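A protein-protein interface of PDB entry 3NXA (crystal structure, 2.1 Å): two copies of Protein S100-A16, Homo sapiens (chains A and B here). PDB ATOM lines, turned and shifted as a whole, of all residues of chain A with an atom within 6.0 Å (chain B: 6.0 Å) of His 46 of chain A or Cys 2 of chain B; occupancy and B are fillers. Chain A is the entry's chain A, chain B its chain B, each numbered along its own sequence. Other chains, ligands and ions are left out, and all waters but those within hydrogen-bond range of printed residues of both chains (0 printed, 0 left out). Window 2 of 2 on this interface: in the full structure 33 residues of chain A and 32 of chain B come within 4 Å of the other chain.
No position is printed for both chains. Of the 8 pairs that touch across the chains among the printed residues, none has its exchanged pair printed and touching as well.
Printed residues of chain B within 4 Å of Asn 45 of chain A: Glu 7. Of the printed residues of chain B, Met 47 of chain A touches Glu 7. Cys 2 of chain B touches just one residue of chain A: His 46. Lys 8 of chain B touches none of the printed residues of chain A. The nearest residue of chain B that does not touch His 46 of chain A is Thr 4 of chain B (4.5 Å). The nearest printed residue of chain B that does not touch Glu 43 of chain A is Tyr 3 of chain B (6.0 Å).
Among the printed residues, merely in contact across the chains: Glu 43 of chain A with Glu 7 of chain B (3.5 Å), Leu 44 of chain A with Glu 7 of chain B (2.9 Å) and His 46 of chain A with Tyr 3 of chain B (3.5 Å).
The backbone carbonyl oxygen (O) of Glu 43 of chain A lies close to the side-chain hydroxyl (OG1) of Thr 4 of chain B (2.2 Å). The side-chain carboxylate of Glu 7 of chain B is in hydrogen-bond range of the backbone NH of Met 47 of chain A (3.1 Å). N of Asn 45 of chain A lies within hydrogen-bond range of OE2 of Glu 7 of chain B, at 3.2 Å. A ring nitrogen (NE2) of His 46 of chain A lies close to the backbone carbonyl oxygen (O) of Cys 2 of chain B (3.4 Å). The backbone NH (N) of His 46 of chain A lies within hydrogen-bond range of the side-chain carboxylate (OE2) of Glu 7 of chain B (2.9 Å).
Of the 5 printed residues of chain B, 4 touch a printed residue of chain A. Hydrophobic or aromatic side chains of chain B that line the printed part of chain A: Tyr 3. Printed residues of chain A that touch a printed residue of chain B: Glu 43, Leu 44, Asn 45, His 46 and Met 47. Hydrophobic or aromatic side chains of chain A within 4 Å of the printed part of chain B: Leu 44, His 46 and Met 47. Among the printed residues, 8 pairs touch across the chains. Among the printed residues, no Asp or Glu carboxylate lies within 4 Å of a Lys or Arg side-chain nitrogen of the other chain.
The side-chain hydroxyl (OG) of Ser 49 of chain A is in hydrogen-bond range of the backbone carbonyl oxygen (O) of His 46 of chain A (3.1 Å). OG1 of Thr 4 of chain B lies within hydrogen-bond range of N of Glu 7 of chain B, at 3.0 Å.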
ATOM      1  N   GLU A  43       6.826  23.609  -6.556  1.00  0.00           N
ATOM      2  CA  GLU A  43       8.247  23.800  -6.016  1.00  0.00           C
ATOM      3  C   GLU A  43       9.097  22.481  -6.077  1.00  0.00           C
ATOM      4  O   GLU A  43      10.389  22.590  -6.233  1.00  0.00           O
ATOM      5  CB  GLU A  43       8.149  24.456  -4.526  1.00  0.00           C
ATOM      6  CG  GLU A  43       7.365  25.838  -4.571  1.00  0.00           C
ATOM      7  CD  GLU A  43       7.969  26.993  -5.434  1.00  0.00           C
ATOM      8  OE1 GLU A  43       9.150  26.957  -5.881  1.00  0.00           O
ATOM      9  OE2 GLU A  43       7.236  28.024  -5.771  1.00  0.00           O
ATOM     10  N   LEU A  44       8.397  21.287  -6.079  1.00  0.00           N
ATOM     11  CA  LEU A  44       9.021  19.971  -6.037  1.00  0.00           C
ATOM     12  C   LEU A  44       8.608  19.112  -7.238  1.00  0.00           C
ATOM     13  O   LEU A  44       8.373  17.869  -7.066  1.00  0.00           O
ATOM     14  CB  LEU A  44       8.561  19.114  -4.858  1.00  0.00           C
ATOM     15  CG  LEU A  44       9.275  19.501  -3.561  1.00  0.00           C
ATOM     16  CD1 LEU A  44       9.057  18.520  -2.463  1.00  0.00           C
ATOM     17  CD2 LEU A  44      10.863  19.909  -3.783  1.00  0.00           C
ATOM     18  N   ASN A  45       8.209  19.747  -8.361  1.00  0.00           N
ATOM     19  CA  ASN A  45       7.625  18.764  -9.293  1.00  0.00           C
ATOM     20  C   ASN A  45       8.719  17.994 -10.143  1.00  0.00           C
ATOM     21  O   ASN A  45       8.349  16.868 -10.641  1.00  0.00           O
ATOM     22  CB  ASN A  45       6.437  19.355  -9.980  1.00  0.00           C
ATOM     23  CG  ASN A  45       6.841  19.958 -11.150  1.00  0.00           C
ATOM     24  OD1 ASN A  45       7.839  20.781 -11.176  1.00  0.00           O
ATOM     25  ND2 ASN A  45       6.228  19.471 -12.237  1.00  0.00           N
ATOM     26  N   HIS A  46      10.034  18.436 -10.140  1.00  0.00           N
ATOM     27  CA  HIS A  46      11.062  17.489 -10.494  1.00  0.00           C
ATOM     28  C   HIS A  46      11.129  16.311  -9.539  1.00  0.00           C
ATOM     29  O   HIS A  46      10.807  15.202  -9.972  1.00  0.00           O
ATOM     30  CB  HIS A  46      12.449  18.051 -10.779  1.00  0.00           C
ATOM     31  CG  HIS A  46      12.414  19.236 -11.724  1.00  0.00           C
ATOM     32  ND1 HIS A  46      11.875  20.477 -11.367  1.00  0.00           N
ATOM     33  CD2 HIS A  46      12.833  19.348 -13.030  1.00  0.00           C
ATOM     34  CE1 HIS A  46      12.107  21.318 -12.367  1.00  0.00           C
ATOM     35  NE2 HIS A  46      12.611  20.644 -13.420  1.00  0.00           N
ATOM     36  N   MET A  47      11.406  16.539  -8.261  1.00  0.00           N
ATOM     37  CA  MET A  47      11.581  15.515  -7.311  1.00  0.00           C
ATOM     38  C   MET A  47      10.300  14.811  -7.125  1.00  0.00           C
ATOM     39  O   MET A  47      10.291  13.647  -6.674  1.00  0.00           O
ATOM     40  CB  MET A  47      12.112  15.944  -5.934  1.00  0.00           C
ATOM     41  CG  MET A  47      13.316  16.801  -6.066  1.00  0.00           C
ATOM     42  SD  MET A  47      14.134  17.235  -4.515  1.00  0.00           S
ATOM     43  CE  MET A  47      13.020  16.285  -3.358  1.00  0.00           C
ATOM     44  N   LEU A  48       9.227  15.371  -7.554  1.00  0.00           N
ATOM     45  CA  LEU A  48       8.016  14.482  -7.442  1.00  0.00           C
ATOM     46  C   LEU A  48       7.394  13.886  -8.832  1.00  0.00           C
ATOM     47  O   LEU A  48       6.151  13.523  -8.919  1.00  0.00           O
ATOM     48  CB  LEU A  48       6.865  15.076  -6.505  1.00  0.00           C
ATOM     49  CG  LEU A  48       6.792  14.795  -4.970  1.00  0.00           C
ATOM     50  CD1 LEU A  48       8.161  14.991  -4.426  1.00  0.00           C
ATOM     51  CD2 LEU A  48       5.984  15.632  -4.318  1.00  0.00           C
ATOM     52  N   SER A  49       8.235  13.740  -9.827  1.00  0.00           N
ATOM     53  CA  SER A  49       7.781  13.010 -10.951  1.00  0.00           C
ATOM     54  C   SER A  49       7.340  11.606 -10.830  1.00  0.00           C
ATOM     55  O   SER A  49       6.535  11.111 -11.575  1.00  0.00           O
ATOM     56  CB  SER A  49       8.615  13.242 -12.163  1.00  0.00           C
ATOM     57  OG  SER A  49       9.948  12.933 -11.941  1.00  0.00           O
ATOM     58  N   ASP A  50       8.102  10.869 -10.046  1.00  0.00           N
ATOM     59  CA  ASP A  50       7.677   9.496 -10.038  1.00  0.00           C
ATOM     60  C   ASP A  50       6.165   9.605  -9.659  1.00  0.00           C
ATOM     61  O   ASP A  50       5.738  10.689 -10.228  1.00  0.00           O
ATOM     62  CB  ASP A  50       8.460   8.450  -9.390  1.00  0.00           C
ATOM     63  CG  ASP A  50       8.260   7.003  -9.612  1.00  0.00           C
ATOM     64  OD1 ASP A  50       7.627   6.538 -10.619  1.00  0.00           O
ATOM     65  OD2 ASP A  50       8.782   6.182  -8.842  1.00  0.00           O
ATOM     66  N   CYS B   2      16.589  24.028 -15.128  1.00  0.00           N
ATOM     67  CA  CYS B   2      16.979  23.290 -13.892  1.00  0.00           C
ATOM     68  C   CYS B   2      15.883  23.074 -12.847  1.00  0.00           C
ATOM     69  O   CYS B   2      14.771  23.296 -13.016  1.00  0.00           O
ATOM     70  CB  CYS B   2      18.081  24.161 -13.167  1.00  0.00           C
ATOM     71  SG  CYS B   2      19.356  23.121 -12.253  1.00  0.00           S
ATOM     72  N   TYR B   3      16.284  22.649 -11.668  1.00  0.00           N
ATOM     73  CA  TYR B   3      15.362  22.459 -10.448  1.00  0.00           C
ATOM     74  C   TYR B   3      15.035  23.793  -9.809  1.00  0.00           C
ATOM     75  O   TYR B   3      15.754  24.848  -9.969  1.00  0.00           O
ATOM     76  CB  TYR B   3      16.115  21.526  -9.505  1.00  0.00           C
ATOM     77  CG  TYR B   3      16.297  20.130  -9.987  1.00  0.00           C
ATOM     78  CD1 TYR B   3      16.843  19.131  -9.175  1.00  0.00           C
ATOM     79  CD2 TYR B   3      15.853  19.759 -11.370  1.00  0.00           C
ATOM     80  CE1 TYR B   3      17.055  17.700  -9.620  1.00  0.00           C
ATOM     81  CE2 TYR B   3      15.968  18.356 -11.856  1.00  0.00           C
ATOM     82  CZ  TYR B   3      16.569  17.298 -11.005  1.00  0.00           C
ATOM     83  OH  TYR B   3      16.608  15.975 -11.629  1.00  0.00           O
ATOM     84  N   THR B   4      13.893  23.835  -9.133  1.00  0.00           N
ATOM     85  CA  THR B   4      13.481  25.053  -8.372  1.00  0.00           C
ATOM     86  C   THR B   4      14.412  25.246  -7.332  1.00  0.00           C
ATOM     87  O   THR B   4      15.254  24.333  -7.028  1.00  0.00           O
ATOM     88  CB  THR B   4      12.120  24.815  -7.690  1.00  0.00           C
ATOM     89  OG1 THR B   4      12.263  23.704  -6.788  1.00  0.00           O
ATOM     90  CG2 THR B   4      10.956  24.457  -8.798  1.00  0.00           C
ATOM     91  N   GLU B   7      13.989  22.672  -4.555  1.00  0.00           N
ATOM     92  CA  GLU B   7      14.742  21.486  -4.841  1.00  0.00           C
ATOM     93  C   GLU B   7      16.164  21.621  -4.629  1.00  0.00           C
ATOM     94  O   GLU B   7      16.808  20.633  -4.127  1.00  0.00           O
ATOM     95  CB  GLU B   7      14.449  20.971  -6.357  1.00  0.00           C
ATOM     96  CG  GLU B   7      13.278  20.215  -6.306  1.00  0.00           C
ATOM     97  CD  GLU B   7      12.551  20.176  -7.720  1.00  0.00           C
ATOM     98  OE1 GLU B   7      13.077  20.885  -8.619  1.00  0.00           O
ATOM     99  OE2 GLU B   7      11.395  19.576  -7.803  1.00  0.00           O
ATOM    100  N   LYS B   8      16.781  22.713  -5.058  1.00  0.00           N
ATOM    101  CA  LYS B   8      18.267  22.632  -5.006  1.00  0.00           C
ATOM    102  C   LYS B   8      18.689  22.750  -3.458  1.00  0.00           C
ATOM    103  O   LYS B   8      19.776  22.314  -2.967  1.00  0.00           O
ATOM    104  CB  LYS B   8      18.754  23.909  -5.497  1.00  0.00           C
ATOM    105  CG  LYS B   8      18.777  23.836  -6.869  1.00  0.00           C
ATOM    106  CD  LYS B   8      19.853  24.926  -7.330  1.00  0.00           C
ATOM    107  CE  LYS B   8      19.327  25.757  -8.408  1.00  0.00           C
ATOM    108  NZ  LYS B   8      19.138  27.162  -7.649  1.00  0.00           N
